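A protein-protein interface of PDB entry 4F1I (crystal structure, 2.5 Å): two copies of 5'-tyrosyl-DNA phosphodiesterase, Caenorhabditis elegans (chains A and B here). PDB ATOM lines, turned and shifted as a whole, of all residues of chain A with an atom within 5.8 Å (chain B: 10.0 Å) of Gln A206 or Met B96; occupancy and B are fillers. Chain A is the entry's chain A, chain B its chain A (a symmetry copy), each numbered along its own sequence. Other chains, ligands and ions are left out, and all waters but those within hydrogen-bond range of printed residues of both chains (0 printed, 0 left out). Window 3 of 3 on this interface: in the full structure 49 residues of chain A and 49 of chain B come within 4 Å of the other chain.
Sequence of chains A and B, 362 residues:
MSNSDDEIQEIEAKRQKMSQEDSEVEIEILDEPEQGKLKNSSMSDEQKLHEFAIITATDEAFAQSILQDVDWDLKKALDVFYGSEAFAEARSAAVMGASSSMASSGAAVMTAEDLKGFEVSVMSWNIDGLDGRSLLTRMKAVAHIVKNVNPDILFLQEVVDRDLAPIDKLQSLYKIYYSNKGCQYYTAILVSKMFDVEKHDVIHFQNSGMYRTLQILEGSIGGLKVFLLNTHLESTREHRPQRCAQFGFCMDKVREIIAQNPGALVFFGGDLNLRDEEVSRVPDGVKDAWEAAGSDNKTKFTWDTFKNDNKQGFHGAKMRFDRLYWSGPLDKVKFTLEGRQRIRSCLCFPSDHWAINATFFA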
ATOM      1  N   ILE A 203     -35.687 -16.873  24.490  1.00  0.00           N
ATOM      2  CA  ILE A 203     -34.425 -17.392  24.998  1.00  0.00           C
ATOM      3  C   ILE A 203     -34.517 -17.629  26.499  1.00  0.00           C
ATOM      4  O   ILE A 203     -34.709 -16.693  27.268  1.00  0.00           O
ATOM      5  CB  ILE A 203     -33.267 -16.413  24.720  1.00  0.00           C
ATOM      6  CG1 ILE A 203     -33.089 -16.221  23.209  1.00  0.00           C
ATOM      7  CG2 ILE A 203     -31.980 -16.911  25.364  1.00  0.00           C
ATOM      8  CD1 ILE A 203     -32.148 -15.093  22.846  1.00  0.00           C
ATOM      9  N   HIS A 204     -34.384 -18.881  26.917  1.00  0.00           N
ATOM     10  CA  HIS A 204     -34.442 -19.204  28.339  1.00  0.00           C
ATOM     11  C   HIS A 204     -33.092 -18.989  29.020  1.00  0.00           C
ATOM     12  O   HIS A 204     -32.105 -19.636  28.677  1.00  0.00           O
ATOM     13  CB  HIS A 204     -34.922 -20.643  28.548  1.00  0.00           C
ATOM     14  CG  HIS A 204     -36.338 -20.871  28.119  1.00  0.00           C
ATOM     15  ND1 HIS A 204     -36.728 -20.856  26.798  1.00  0.00           N
ATOM     16  CD2 HIS A 204     -37.459 -21.112  28.841  1.00  0.00           C
ATOM     17  CE1 HIS A 204     -38.028 -21.081  26.722  1.00  0.00           C
ATOM     18  NE2 HIS A 204     -38.494 -21.240  27.946  1.00  0.00           N
ATOM     19  N   PHE A 205     -33.056 -18.072  29.979  1.00  0.00           N
ATOM     20  CA  PHE A 205     -31.849 -17.850  30.769  1.00  0.00           C
ATOM     21  C   PHE A 205     -31.502 -19.102  31.566  1.00  0.00           C
ATOM     22  O   PHE A 205     -32.294 -19.554  32.395  1.00  0.00           O
ATOM     23  CB  PHE A 205     -32.048 -16.680  31.731  1.00  0.00           C
ATOM     24  CG  PHE A 205     -32.279 -15.363  31.053  1.00  0.00           C
ATOM     25  CD1 PHE A 205     -31.698 -15.084  29.828  1.00  0.00           C
ATOM     26  CD2 PHE A 205     -33.077 -14.402  31.649  1.00  0.00           C
ATOM     27  CE1 PHE A 205     -31.908 -13.865  29.210  1.00  0.00           C
ATOM     28  CE2 PHE A 205     -33.296 -13.184  31.036  1.00  0.00           C
ATOM     29  CZ  PHE A 205     -32.708 -12.913  29.816  1.00  0.00           C
ATOM     30  N   GLN A 206     -30.322 -19.660  31.323  1.00  0.00           N
ATOM     31  CA  GLN A 206     -29.934 -20.905  31.984  1.00  0.00           C
ATOM     32  C   GLN A 206     -29.417 -20.678  33.405  1.00  0.00           C
ATOM     33  O   GLN A 206     -29.350 -21.611  34.202  1.00  0.00           O
ATOM     34  CB  GLN A 206     -28.900 -21.665  31.151  1.00  0.00           C
ATOM     35  CG  GLN A 206     -29.172 -23.157  31.045  1.00  0.00           C
ATOM     36  CD  GLN A 206     -30.426 -23.479  30.239  1.00  0.00           C
ATOM     37  OE1 GLN A 206     -30.960 -22.628  29.519  1.00  0.00           O
ATOM     38  NE2 GLN A 206     -30.900 -24.717  30.357  1.00  0.00           N
ATOM     39  N   ASN A 207     -29.059 -19.438  33.716  1.00  0.00           N
ATOM     40  CA  ASN A 207     -28.590 -19.103  35.051  1.00  0.00           C
ATOM     41  C   ASN A 207     -29.744 -18.677  35.960  1.00  0.00           C
ATOM     42  O   ASN A 207     -29.531 -18.177  37.063  1.00  0.00           O
ATOM     43  CB  ASN A 207     -27.521 -18.007  34.984  1.00  0.00           C
ATOM     44  CG  ASN A 207     -28.101 -16.638  34.681  1.00  0.00           C
ATOM     45  OD1 ASN A 207     -29.132 -16.515  34.015  1.00  0.00           O
ATOM     46  ND2 ASN A 207     -27.438 -15.598  35.171  1.00  0.00           N
ATOM     47  N   SER A 208     -30.967 -18.881  35.485  1.00  0.00           N
ATOM     48  CA  SER A 208     -32.149 -18.428  36.205  1.00  0.00           C
ATOM     49  C   SER A 208     -32.829 -19.570  36.944  1.00  0.00           C
ATOM     50  O   SER A 208     -33.050 -20.637  36.377  1.00  0.00           O
ATOM     51  CB  SER A 208     -33.143 -17.778  35.238  1.00  0.00           C
ATOM     52  OG  SER A 208     -34.362 -17.459  35.894  1.00  0.00           O
ATOM     53  N   PHE A 249     -26.089  -9.415  28.946  1.00  0.00           N
ATOM     54  CA  PHE A 249     -26.362 -10.385  27.897  1.00  0.00           C
ATOM     55  C   PHE A 249     -27.479  -9.874  26.988  1.00  0.00           C
ATOM     56  O   PHE A 249     -27.415 -10.015  25.768  1.00  0.00           O
ATOM     57  CB  PHE A 249     -26.749 -11.727  28.525  1.00  0.00           C
ATOM     58  CG  PHE A 249     -27.342 -12.710  27.560  1.00  0.00           C
ATOM     59  CD1 PHE A 249     -26.530 -13.463  26.731  1.00  0.00           C
ATOM     60  CD2 PHE A 249     -28.713 -12.890  27.491  1.00  0.00           C
ATOM     61  CE1 PHE A 249     -27.076 -14.372  25.845  1.00  0.00           C
ATOM     62  CE2 PHE A 249     -29.266 -13.794  26.607  1.00  0.00           C
ATOM     63  CZ  PHE A 249     -28.446 -14.540  25.785  1.00  0.00           C
ATOM     64  N   ALA B  88     -18.636 -10.513  25.622  1.00  0.00           N
ATOM     65  CA  ALA B  88     -19.946 -11.033  25.244  1.00  0.00           C
ATOM     66  C   ALA B  88     -19.983 -12.550  25.385  1.00  0.00           C
ATOM     67  O   ALA B  88     -20.867 -13.103  26.048  1.00  0.00           O
ATOM     68  CB  ALA B  88     -20.289 -10.624  23.825  1.00  0.00           C
ATOM     69  N   GLU B  89     -18.991 -13.202  24.784  1.00  0.00           N
ATOM     70  CA  GLU B  89     -18.818 -14.646  24.874  1.00  0.00           C
ATOM     71  C   GLU B  89     -18.950 -15.112  26.319  1.00  0.00           C
ATOM     72  O   GLU B  89     -19.807 -15.945  26.640  1.00  0.00           O
ATOM     73  CB  GLU B  89     -17.447 -15.041  24.323  1.00  0.00           C
ATOM     74  CG  GLU B  89     -17.248 -16.533  24.119  1.00  0.00           C
ATOM     75  CD  GLU B  89     -17.743 -17.012  22.765  1.00  0.00           C
ATOM     76  OE1 GLU B  89     -18.586 -16.319  22.152  1.00  0.00           O
ATOM     77  OE2 GLU B  89     -17.276 -18.081  22.309  1.00  0.00           O
ATOM     78  N   ALA B  90     -18.122 -14.541  27.190  1.00  0.00           N
ATOM     79  CA  ALA B  90     -18.143 -14.885  28.604  1.00  0.00           C
ATOM     80  C   ALA B  90     -19.554 -14.737  29.153  1.00  0.00           C
ATOM     81  O   ALA B  90     -20.088 -15.660  29.777  1.00  0.00           O
ATOM     82  CB  ALA B  90     -17.174 -14.011  29.381  1.00  0.00           C
ATOM     83  N   ARG B  91     -20.169 -13.590  28.875  1.00  0.00           N
ATOM     84  CA  ARG B  91     -21.512 -13.326  29.369  1.00  0.00           C
ATOM     85  C   ARG B  91     -22.477 -14.388  28.869  1.00  0.00           C
ATOM     86  O   ARG B  91     -23.309 -14.883  29.633  1.00  0.00           O
ATOM     87  CB  ARG B  91     -21.984 -11.924  28.979  1.00  0.00           C
ATOM     88  CG  ARG B  91     -21.362 -10.823  29.821  1.00  0.00           C
ATOM     89  CD  ARG B  91     -22.011  -9.479  29.555  1.00  0.00           C
ATOM     90  NE  ARG B  91     -21.781  -9.027  28.187  1.00  0.00           N
ATOM     91  CZ  ARG B  91     -20.698  -8.366  27.790  1.00  0.00           C
ATOM     92  NH1 ARG B  91     -19.739  -8.075  28.659  1.00  0.00           N
ATOM     93  NH2 ARG B  91     -20.576  -7.996  26.524  1.00  0.00           N
ATOM     94  N   SER B  92     -22.340 -14.763  27.598  1.00  0.00           N
ATOM     95  CA  SER B  92     -23.191 -15.802  27.038  1.00  0.00           C
ATOM     96  C   SER B  92     -22.994 -17.068  27.859  1.00  0.00           C
ATOM     97  O   SER B  92     -23.960 -17.665  28.340  1.00  0.00           O
ATOM     98  CB  SER B  92     -22.857 -16.054  25.567  1.00  0.00           C
ATOM     99  OG  SER B  92     -23.783 -16.958  24.989  1.00  0.00           O
ATOM    100  N   ALA B  93     -21.730 -17.434  28.061  1.00  0.00           N
ATOM    101  CA  ALA B  93     -21.385 -18.616  28.837  1.00  0.00           C
ATOM    102  C   ALA B  93     -21.952 -18.516  30.247  1.00  0.00           C
ATOM    103  O   ALA B  93     -22.311 -19.525  30.857  1.00  0.00           O
ATOM    104  CB  ALA B  93     -19.871 -18.801  28.880  1.00  0.00           C
ATOM    105  N   ALA B  94     -22.045 -17.293  30.759  1.00  0.00           N
ATOM    106  CA  ALA B  94     -22.531 -17.091  32.115  1.00  0.00           C
ATOM    107  C   ALA B  94     -24.045 -17.232  32.174  1.00  0.00           C
ATOM    108  O   ALA B  94     -24.596 -17.673  33.183  1.00  0.00           O
ATOM    109  CB  ALA B  94     -22.099 -15.732  32.634  1.00  0.00           C
ATOM    110  N   VAL B  95     -24.719 -16.871  31.086  1.00  0.00           N
ATOM    111  CA  VAL B  95     -26.176 -16.878  31.086  1.00  0.00           C
ATOM    112  C   VAL B  95     -26.729 -18.142  30.440  1.00  0.00           C
ATOM    113  O   VAL B  95     -27.716 -18.708  30.910  1.00  0.00           O
ATOM    114  CB  VAL B  95     -26.750 -15.629  30.378  1.00  0.00           C
ATOM    115  CG1 VAL B  95     -28.268 -15.664  30.377  1.00  0.00           C
ATOM    116  CG2 VAL B  95     -26.255 -14.367  31.058  1.00  0.00           C
ATOM    117  N   MET B  96     -26.073 -18.597  29.379  1.00  0.00           N
ATOM    118  CA  MET B  96     -26.588 -19.708  28.586  1.00  0.00           C
ATOM    119  C   MET B  96     -25.824 -21.014  28.777  1.00  0.00           C
ATOM    120  O   MET B  96     -26.282 -22.075  28.351  1.00  0.00           O
ATOM    121  CB  MET B  96     -26.618 -19.321  27.107  1.00  0.00           C
ATOM    122  CG  MET B  96     -27.581 -18.189  26.813  1.00  0.00           C
ATOM    123  SD  MET B  96     -29.328 -18.611  27.547  1.00  0.00           S
ATOM    124  CE  MET B  96     -29.669 -20.251  26.541  1.00  0.00           C
ATOM    125  N   GLY B  97     -24.666 -20.938  29.424  1.00  0.00           N
ATOM    126  CA  GLY B  97     -23.817 -22.102  29.590  1.00  0.00           C
ATOM    127  C   GLY B  97     -23.069 -22.408  28.308  1.00  0.00           C
ATOM    128  O   GLY B  97     -22.702 -21.495  27.565  1.00  0.00           O
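O of Val B95 is in hydrogen-bond range of N of Asn A207, 3.2 Å away. SD of Met B96 sits close to O of His A204 (3.2 Å). O of Val B95 is in hydrogen-bond range of N of Gln A206, 2.8 Å away.
The backbone carbonyl oxygen (O) of His A204 lies close to the side-chain amide oxygen (OE1) of Gln A206.
Met B96 touches Ile A203. Phe A205 touches Val B95 (CD1 to CG1, 3.5 Å). Met B96 touches Gln A206. Ala B94 touches Asn A207. CB of Phe A249 touches CG2 of Val B95 (3.7 Å). Met B96 touches Phe A249.
Of the printed residues of chain B, Gln A206 touches Val B95 (2.8 Å) and Met B96 (3.9 Å). Of the printed residues of chain A, Met B96 touches Ile A203 (3.8 Å), His A204 (3.2 Å), Gln A206 (3.9 Å) and Phe A249 (3.9 Å). Asn A207 touches just these residues of chain B: Ala B94 and Val B95. Printed residues of chain B within 4 Å of Phe A249: Val B95 and Met B96. Printed residues of chain B within 4 Å of Ile A203: Met B96 (3.8 Å). Of the printed residues of chain B, Phe A205 touches Val B95. The nearest residue of chain A that does not touch Met B96 is Phe A205 (4.2 Å). The nearest printed residue of chain A that does not touch Val B95 is His A204 (5.0 Å).
Printed residues of chain A that touch a printed residue of chain B: Ile A203, His A204, Phe A205, Gln A206, Asn A207 and Phe A249. Hydrophobic or aromatic side chains of chain A that line the printed part of chain B: Ile A203, Phe A205 and Phe A249. Hydrophobic or aromatic side chains of chain B that line the printed part of chain A: Val B95 and Met B96. Along chain B the printed residues that touch a printed residue of chain A span positions 94 to 96. Among the printed residues, 9 pairs touch across the chains. Among the printed residues, no Asp or Glu carboxylate lies within 4 Å of a Lys or Arg side-chain nitrogen of the other chain.
No position is printed for both chains.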
